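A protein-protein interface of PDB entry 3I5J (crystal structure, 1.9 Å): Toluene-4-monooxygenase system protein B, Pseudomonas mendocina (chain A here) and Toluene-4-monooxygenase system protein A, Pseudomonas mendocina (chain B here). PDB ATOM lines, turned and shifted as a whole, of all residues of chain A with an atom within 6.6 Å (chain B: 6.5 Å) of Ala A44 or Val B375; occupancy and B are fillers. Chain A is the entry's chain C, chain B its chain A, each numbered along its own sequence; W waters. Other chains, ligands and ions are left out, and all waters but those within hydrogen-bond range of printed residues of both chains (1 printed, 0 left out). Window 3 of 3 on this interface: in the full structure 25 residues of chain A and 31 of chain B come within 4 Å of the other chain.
Ala A44 touches just one residue of chain B: Val B375.
Printed residues of chain A within 4 Å of Val B375: Asn A40 (3.4 Å), Arg A41 (3.3 Å), Arg A42 (3.996 Å), Val A43 (3.95 Å) and Ala A44 (3.8 Å).
Of the printed residues of chain A, Ile B376 touches Arg A41 (3.5 Å).
Of the printed residues of chain B, Arg A42 touches Cys B372 and Val B375.
Of the printed residues of chain B, Asn A40 touches Val B375 and Asn B379.
Val A39 touches none of the printed residues of chain B.
The nearest printed residue of chain B that does not touch Arg A41 is Asn B379 (4.2 Å).
O of Val B375 lies close to OD1 of Asn B379.
N of Arg B384 lies within hydrogen-bond range of O of Asn B379 (2.7 Å).
N of Val A43 sits at hydrogen-bond distance from O of Cys A38.
Among the printed residues, pairs that only touch across the chains: Asn A40 with Val B375 (3.4 Å), Arg A41 with Val B375 (3.3 Å), Arg A41 with Ile B376 (3.5 Å), Arg A42 with Val B375 (3.996 Å), Val A43 with Val B375 (3.95 Å) and Ala A44 with Val B375 (3.8 Å).
Water W1 bridges OD1 of Asn B379 (2.7 Å) and O of Arg A41 (2.8 Å).
Of the 12 printed residues of chain A, 5 touch a printed residue of chain B.
Hydrophobic or aromatic side chains of chain B that line the printed part of chain A: Val B375 and Ile B376.
The side-chain sulfur of Cys B372 sits close to the backbone carbonyl oxygen of Arg A42 (3.4 Å).
The backbone carbonyl oxygen (O) of Asn A40 lies close to the side-chain amide oxygen (OD1) of Asn B379 (2.8 Å).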
ATOM      1  N   PHE A  10      -3.524   1.744  11.258  1.00  0.00           N
ATOM      2  CA  PHE A  10      -4.387   0.927  10.369  1.00  0.00           C
ATOM      3  C   PHE A  10      -5.665   1.671  10.044  1.00  0.00           C
ATOM      4  O   PHE A  10      -6.258   2.286  10.962  1.00  0.00           O
ATOM      5  CB  PHE A  10      -4.754  -0.363  11.028  1.00  0.00           C
ATOM      6  CG  PHE A  10      -5.265  -1.401  10.095  1.00  0.00           C
ATOM      7  CD1 PHE A  10      -6.604  -1.417   9.752  1.00  0.00           C
ATOM      8  CD2 PHE A  10      -4.402  -2.327   9.561  1.00  0.00           C
ATOM      9  CE1 PHE A  10      -7.110  -2.425   8.889  1.00  0.00           C
ATOM     10  CE2 PHE A  10      -4.862  -3.329   8.729  1.00  0.00           C
ATOM     11  CZ  PHE A  10      -6.209  -3.359   8.351  1.00  0.00           C
ATOM     12  N   LYS A  12      -9.141   3.050   9.903  1.00  0.00           N
ATOM     13  CA  LYS A  12     -10.393   3.128  10.695  1.00  0.00           C
ATOM     14  C   LYS A  12     -10.154   2.877  12.199  1.00  0.00           C
ATOM     15  O   LYS A  12     -11.083   3.004  13.003  1.00  0.00           O
ATOM     16  CB  LYS A  12     -11.469   2.181  10.115  1.00  0.00           C
ATOM     17  CG  LYS A  12     -12.042   2.740   8.820  1.00  0.00           C
ATOM     18  CD  LYS A  12     -13.053   1.818   8.206  1.00  0.00           C
ATOM     19  CE  LYS A  12     -13.721   2.538   7.038  1.00  0.00           C
ATOM     20  NZ  LYS A  12     -15.144   2.392   7.300  1.00  0.00           N
ATOM     21  N   CYS A  38      -5.059  -5.248  14.990  1.00  0.00           N
ATOM     22  CA  CYS A  38      -6.098  -4.263  14.662  1.00  0.00           C
ATOM     23  C   CYS A  38      -7.429  -4.860  14.251  1.00  0.00           C
ATOM     24  O   CYS A  38      -8.488  -4.535  14.801  1.00  0.00           O
ATOM     25  CB  CYS A  38      -5.645  -3.374  13.499  1.00  0.00           C
ATOM     26  SG  CYS A  38      -4.209  -2.382  13.839  1.00  0.00           S
ATOM     27  N   VAL A  39      -7.370  -5.642  13.176  1.00  0.00           N
ATOM     28  CA  VAL A  39      -8.564  -6.171  12.601  1.00  0.00           C
ATOM     29  C   VAL A  39      -9.126  -7.188  13.595  1.00  0.00           C
ATOM     30  O   VAL A  39      -8.415  -8.019  14.146  1.00  0.00           O
ATOM     31  CB  VAL A  39      -8.297  -6.763  11.159  1.00  0.00           C
ATOM     32  CG1 VAL A  39      -9.380  -7.641  10.729  1.00  0.00           C
ATOM     33  CG2 VAL A  39      -8.075  -5.584  10.163  1.00  0.00           C
ATOM     34  N   ASN A  40     -10.411  -7.011  13.890  1.00  0.00           N
ATOM     35  CA  ASN A  40     -11.160  -7.907  14.821  1.00  0.00           C
ATOM     36  C   ASN A  40     -10.798  -7.605  16.283  1.00  0.00           C
ATOM     37  O   ASN A  40     -11.127  -8.383  17.167  1.00  0.00           O
ATOM     38  CB  ASN A  40     -10.956  -9.386  14.516  1.00  0.00           C
ATOM     39  CG  ASN A  40     -11.822  -9.873  13.358  1.00  0.00           C
ATOM     40  OD1 ASN A  40     -13.022  -9.560  13.284  1.00  0.00           O
ATOM     41  ND2 ASN A  40     -11.229 -10.628  12.451  1.00  0.00           N
ATOM     42  N   ARG A  41     -10.072  -6.504  16.498  1.00  0.00           N
ATOM     43  CA  ARG A  41      -9.806  -5.990  17.816  1.00  0.00           C
ATOM     44  C   ARG A  41     -10.520  -4.683  17.931  1.00  0.00           C
ATOM     45  O   ARG A  41     -11.367  -4.522  18.825  1.00  0.00           O
ATOM     46  CB  ARG A  41      -8.316  -5.744  18.066  1.00  0.00           C
ATOM     47  CG  ARG A  41      -7.554  -7.092  18.144  1.00  0.00           C
ATOM     48  CD  ARG A  41      -6.121  -6.849  18.416  1.00  0.00           C
ATOM     49  NE  ARG A  41      -5.380  -8.113  18.387  1.00  0.00           N
ATOM     50  CZ  ARG A  41      -5.035  -8.784  19.465  1.00  0.00           C
ATOM     51  NH1 ARG A  41      -5.332  -8.304  20.667  1.00  0.00           N
ATOM     52  NH2 ARG A  41      -4.331  -9.880  19.348  1.00  0.00           N
ATOM     53  N   ARG A  42     -10.154  -3.744  17.033  1.00  0.00           N
ATOM     54  CA  ARG A  42     -10.845  -2.436  17.079  1.00  0.00           C
ATOM     55  C   ARG A  42     -11.427  -2.036  15.731  1.00  0.00           C
ATOM     56  O   ARG A  42     -12.158  -1.035  15.664  1.00  0.00           O
ATOM     57  CB  ARG A  42      -9.900  -1.346  17.653  1.00  0.00           C
ATOM     58  CG  ARG A  42      -9.462  -1.665  19.108  1.00  0.00           C
ATOM     59  CD  ARG A  42      -8.485  -0.569  19.585  1.00  0.00           C
ATOM     60  NE  ARG A  42      -7.445  -0.559  18.589  1.00  0.00           N
ATOM     61  CZ  ARG A  42      -6.468  -1.460  18.570  1.00  0.00           C
ATOM     62  NH1 ARG A  42      -5.597  -1.452  17.585  1.00  0.00           N
ATOM     63  NH2 ARG A  42      -6.381  -2.355  19.532  1.00  0.00           N
ATOM     64  N   VAL A  43     -11.204  -2.886  14.721  1.00  0.00           N
ATOM     65  CA  VAL A  43     -11.492  -2.605  13.343  1.00  0.00           C
ATOM     66  C   VAL A  43     -12.136  -3.799  12.675  1.00  0.00           C
ATOM     67  O   VAL A  43     -11.584  -4.922  12.721  1.00  0.00           O
ATOM     68  CB  VAL A  43     -10.187  -2.289  12.633  1.00  0.00           C
ATOM     69  CG1 VAL A  43     -10.388  -2.208  11.154  1.00  0.00           C
ATOM     70  CG2 VAL A  43      -9.572  -0.959  13.265  1.00  0.00           C
ATOM     71  N   ALA A  44     -13.305  -3.562  12.072  1.00  0.00           N
ATOM     72  CA  ALA A  44     -14.110  -4.667  11.499  1.00  0.00           C
ATOM     73  C   ALA A  44     -13.507  -5.244  10.223  1.00  0.00           C
ATOM     74  O   ALA A  44     -13.042  -4.497   9.359  1.00  0.00           O
ATOM     75  CB  ALA A  44     -15.529  -4.192  11.238  1.00  0.00           C
ATOM     76  N   PRO A  45     -13.581  -6.569  10.045  1.00  0.00           N
ATOM     77  CA  PRO A  45     -12.917  -7.082   8.842  1.00  0.00           C
ATOM     78  C   PRO A  45     -13.668  -6.617   7.601  1.00  0.00           C
ATOM     79  O   PRO A  45     -14.796  -6.159   7.706  1.00  0.00           O
ATOM     80  CB  PRO A  45     -12.987  -8.599   9.020  1.00  0.00           C
ATOM     81  CG  PRO A  45     -14.220  -8.842   9.900  1.00  0.00           C
ATOM     82  CD  PRO A  45     -14.435  -7.575  10.709  1.00  0.00           C
ATOM     83  N   ARG A  46     -13.032  -6.696   6.437  1.00  0.00           N
ATOM     84  CA  ARG A  46     -13.673  -6.332   5.154  1.00  0.00           C
ATOM     85  C   ARG A  46     -12.915  -6.902   3.981  1.00  0.00           C
ATOM     86  O   ARG A  46     -11.708  -7.186   4.068  1.00  0.00           O
ATOM     87  CB  ARG A  46     -13.782  -4.820   4.945  1.00  0.00           C
ATOM     88  CG  ARG A  46     -12.488  -4.024   5.303  1.00  0.00           C
ATOM     89  CD  ARG A  46     -12.453  -2.630   4.634  1.00  0.00           C
ATOM     90  NE  ARG A  46     -12.378  -2.729   3.180  1.00  0.00           N
ATOM     91  CZ  ARG A  46     -12.190  -1.695   2.354  1.00  0.00           C
ATOM     92  NH1 ARG A  46     -12.137  -1.897   1.038  1.00  0.00           N
ATOM     93  NH2 ARG A  46     -12.045  -0.462   2.841  1.00  0.00           N
ATOM     94  N   PHE A  82      -6.736   0.429   2.479  1.00  0.00           N
ATOM     95  CA  PHE A  82      -7.390  -0.418   1.474  1.00  0.00           C
ATOM     96  C   PHE A  82      -7.494   0.266   0.103  1.00  0.00           C
ATOM     97  O   PHE A  82      -7.819   1.447   0.012  1.00  0.00           O
ATOM     98  CB  PHE A  82      -8.777  -0.820   1.952  1.00  0.00           C
ATOM     99  CG  PHE A  82      -8.760  -1.927   2.970  1.00  0.00           C
ATOM    100  CD1 PHE A  82      -8.815  -3.247   2.573  1.00  0.00           C
ATOM    101  CD2 PHE A  82      -8.684  -1.649   4.325  1.00  0.00           C
ATOM    102  CE1 PHE A  82      -8.805  -4.271   3.509  1.00  0.00           C
ATOM    103  CE2 PHE A  82      -8.671  -2.694   5.270  1.00  0.00           C
ATOM    104  CZ  PHE A  82      -8.725  -4.000   4.844  1.00  0.00           C
ATOM    105  N   GLY B 370     -17.683   4.671  18.327  1.00  0.00           N
ATOM    106  CA  GLY B 370     -18.639   3.589  18.347  1.00  0.00           C
ATOM    107  C   GLY B 370     -18.268   2.405  17.471  1.00  0.00           C
ATOM    108  O   GLY B 370     -18.652   1.244  17.758  1.00  0.00           O
ATOM    109  N   ARG B 371     -17.600   2.681  16.354  1.00  0.00           N
ATOM    110  CA  ARG B 371     -17.195   1.582  15.455  1.00  0.00           C
ATOM    111  C   ARG B 371     -16.202   0.631  16.114  1.00  0.00           C
ATOM    112  O   ARG B 371     -16.304  -0.598  15.930  1.00  0.00           O
ATOM    113  CB  ARG B 371     -16.600   2.095  14.114  1.00  0.00           C
ATOM    114  CG  ARG B 371     -17.611   2.861  13.215  1.00  0.00           C
ATOM    115  CD  ARG B 371     -18.934   2.095  12.945  1.00  0.00           C
ATOM    116  NE  ARG B 371     -19.706   2.820  11.936  1.00  0.00           N
ATOM    117  CZ  ARG B 371     -20.989   2.639  11.685  1.00  0.00           C
ATOM    118  NH1 ARG B 371     -21.677   1.724  12.359  1.00  0.00           N
ATOM    119  NH2 ARG B 371     -21.573   3.372  10.746  1.00  0.00           N
ATOM    120  N   CYS B 372     -15.239   1.186  16.856  1.00  0.00           N
ATOM    121  CA  CYS B 372     -14.274   0.410  17.656  1.00  0.00           C
ATOM    122  C   CYS B 372     -14.938  -0.380  18.801  1.00  0.00           C
ATOM    123  O   CYS B 372     -14.656  -1.558  19.061  1.00  0.00           O
ATOM    124  CB  CYS B 372     -13.238   1.354  18.245  1.00  0.00           C
ATOM    125  SG  CYS B 372     -12.300   2.130  16.934  1.00  0.00           S
ATOM    126  N   TRP B 373     -15.821   0.294  19.499  1.00  0.00           N
ATOM    127  CA  TRP B 373     -16.489  -0.320  20.621  1.00  0.00           C
ATOM    128  C   TRP B 373     -17.472  -1.391  20.181  1.00  0.00           C
ATOM    129  O   TRP B 373     -17.815  -2.257  20.983  1.00  0.00           O
ATOM    130  CB  TRP B 373     -17.210   0.769  21.398  1.00  0.00           C
ATOM    131  CG  TRP B 373     -16.248   1.629  22.200  1.00  0.00           C
ATOM    132  CD1 TRP B 373     -15.973   2.965  22.001  1.00  0.00           C
ATOM    133  CD2 TRP B 373     -15.406   1.208  23.298  1.00  0.00           C
ATOM    134  NE1 TRP B 373     -15.051   3.406  22.939  1.00  0.00           N
ATOM    135  CE2 TRP B 373     -14.663   2.350  23.725  1.00  0.00           C
ATOM    136  CE3 TRP B 373     -15.223  -0.009  23.977  1.00  0.00           C
ATOM    137  CZ2 TRP B 373     -13.766   2.304  24.816  1.00  0.00           C
ATOM    138  CZ3 TRP B 373     -14.324  -0.071  25.012  1.00  0.00           C
ATOM    139  CH2 TRP B 373     -13.594   1.087  25.440  1.00  0.00           C
ATOM    140  N   ASP B 374     -17.934  -1.330  18.936  1.00  0.00           N
ATOM    141  CA  ASP B 374     -18.766  -2.413  18.362  1.00  0.00           C
ATOM    142  C   ASP B 374     -17.979  -3.745  18.266  1.00  0.00           C
ATOM    143  O   ASP B 374     -18.434  -4.818  18.672  1.00  0.00           O
ATOM    144  CB  ASP B 374     -19.347  -2.026  16.986  1.00  0.00           C
ATOM    145  CG  ASP B 374     -20.556  -1.041  17.089  1.00  0.00           C
ATOM    146  OD1 ASP B 374     -21.221  -0.994  18.172  1.00  0.00           O
ATOM    147  OD2 ASP B 374     -20.814  -0.272  16.113  1.00  0.00           O
ATOM    148  N   VAL B 375     -16.770  -3.656  17.755  1.00  0.00           N
ATOM    149  CA  VAL B 375     -15.881  -4.836  17.661  1.00  0.00           C
ATOM    150  C   VAL B 375     -15.533  -5.373  19.037  1.00  0.00           C
ATOM    151  O   VAL B 375     -15.698  -6.561  19.282  1.00  0.00           O
ATOM    152  CB  VAL B 375     -14.597  -4.505  16.830  1.00  0.00           C
ATOM    153  CG1 VAL B 375     -13.631  -5.691  16.738  1.00  0.00           C
ATOM    154  CG2 VAL B 375     -14.973  -3.992  15.417  1.00  0.00           C
ATOM    155  N   ILE B 376     -15.093  -4.495  19.946  1.00  0.00           N
ATOM    156  CA  ILE B 376     -14.684  -4.912  21.277  1.00  0.00           C
ATOM    157  C   ILE B 376     -15.828  -5.579  21.955  1.00  0.00           C
ATOM    158  O   ILE B 376     -15.680  -6.631  22.538  1.00  0.00           O
ATOM    159  CB  ILE B 376     -14.223  -3.712  22.136  1.00  0.00           C
ATOM    160  CG1 ILE B 376     -12.845  -3.179  21.649  1.00  0.00           C
ATOM    161  CG2 ILE B 376     -14.200  -4.083  23.639  1.00  0.00           C
ATOM    162  CD1 ILE B 376     -12.534  -1.702  22.153  1.00  0.00           C
ATOM    163  N   THR B 377     -16.997  -4.934  21.906  1.00  0.00           N
ATOM    164  CA  THR B 377     -18.164  -5.430  22.618  1.00  0.00           C
ATOM    165  C   THR B 377     -18.579  -6.792  22.091  1.00  0.00           C
ATOM    166  O   THR B 377     -18.993  -7.681  22.858  1.00  0.00           O
ATOM    167  CB  THR B 377     -19.369  -4.474  22.509  1.00  0.00           C
ATOM    168  OG1 THR B 377     -19.052  -3.161  23.016  1.00  0.00           O
ATOM    169  CG2 THR B 377     -20.535  -5.054  23.307  1.00  0.00           C
ATOM    170  N   GLU B 378     -18.498  -6.966  20.774  1.00  0.00           N
ATOM    171  CA  GLU B 378     -18.774  -8.274  20.137  1.00  0.00           C
ATOM    172  C   GLU B 378     -17.780  -9.354  20.596  1.00  0.00           C
ATOM    173  O   GLU B 378     -18.143 -10.502  20.805  1.00  0.00           O
ATOM    174  CB  GLU B 378     -18.755  -8.163  18.613  1.00  0.00           C
ATOM    175  CG  GLU B 378     -17.306  -8.492  18.060  1.00  0.00           C
ATOM    176  CD  GLU B 378     -16.995  -8.059  16.609  1.00  0.00           C
ATOM    177  OE1 GLU B 378     -17.891  -7.531  15.894  1.00  0.00           O
ATOM    178  OE2 GLU B 378     -15.824  -8.259  16.183  1.00  0.00           O
ATOM    179  N   ASN B 379     -16.506  -8.988  20.766  1.00  0.00           N
ATOM    180  CA  ASN B 379     -15.552  -9.996  21.244  1.00  0.00           C
ATOM    181  C   ASN B 379     -15.897 -10.394  22.678  1.00  0.00           C
ATOM    182  O   ASN B 379     -15.798 -11.573  23.023  1.00  0.00           O
ATOM    183  CB  ASN B 379     -14.116  -9.527  21.178  1.00  0.00           C
ATOM    184  CG  ASN B 379     -13.603  -9.400  19.765  1.00  0.00           C
ATOM    185  OD1 ASN B 379     -12.849  -8.461  19.426  1.00  0.00           O
ATOM    186  ND2 ASN B 379     -13.962 -10.330  18.947  1.00  0.00           N
ATOM    187  N   VAL B 380     -16.272  -9.411  23.523  1.00  0.00           N
ATOM    188  CA  VAL B 380     -16.651  -9.722  24.912  1.00  0.00           C
ATOM    189  C   VAL B 380     -17.897 -10.618  24.961  1.00  0.00           C
ATOM    190  O   VAL B 380     -17.989 -11.585  25.729  1.00  0.00           O
ATOM    191  CB  VAL B 380     -16.912  -8.455  25.705  1.00  0.00           C
ATOM    192  CG1 VAL B 380     -17.336  -8.780  27.174  1.00  0.00           C
ATOM    193  CG2 VAL B 380     -15.671  -7.563  25.655  1.00  0.00           C
ATOM    194  N   ARG B 384     -14.324 -13.848  23.318  1.00  0.00           N
ATOM    195  CA  ARG B 384     -12.997 -13.845  22.723  1.00  0.00           C
ATOM    196  C   ARG B 384     -12.113 -12.849  23.447  1.00  0.00           C
ATOM    197  O   ARG B 384     -11.790 -11.810  22.889  1.00  0.00           O
ATOM    198  CB  ARG B 384     -13.041 -13.480  21.250  1.00  0.00           C
ATOM    199  CG  ARG B 384     -13.818 -14.450  20.363  1.00  0.00           C
ATOM    200  CD  ARG B 384     -14.005 -13.741  19.024  1.00  0.00           C
ATOM    201  NE  ARG B 384     -15.240 -14.124  18.351  1.00  0.00           N
ATOM    202  CZ  ARG B 384     -16.201 -13.292  17.941  1.00  0.00           C
ATOM    203  NH1 ARG B 384     -16.095 -11.968  18.095  1.00  0.00           N
ATOM    204  NH2 ARG B 384     -17.270 -13.824  17.337  1.00  0.00           N
ATOM    205  N   VAL B 388      -9.108  -8.602  23.308  1.00  0.00           N
ATOM    206  CA  VAL B 388      -9.472  -7.450  24.160  1.00  0.00           C
ATOM    207  C   VAL B 388      -8.294  -7.028  25.026  1.00  0.00           C
ATOM    208  O   VAL B 388      -8.353  -6.103  25.829  1.00  0.00           O
ATOM    209  CB  VAL B 388     -10.726  -7.836  24.963  1.00  0.00           C
ATOM    210  CG1 VAL B 388     -11.160  -6.771  25.768  1.00  0.00           C
ATOM    211  CG2 VAL B 388     -11.844  -8.177  23.940  1.00  0.00           C
HETATM  212  O   HOH W   1     -12.074  -6.315  20.883  1.00  0.00           O
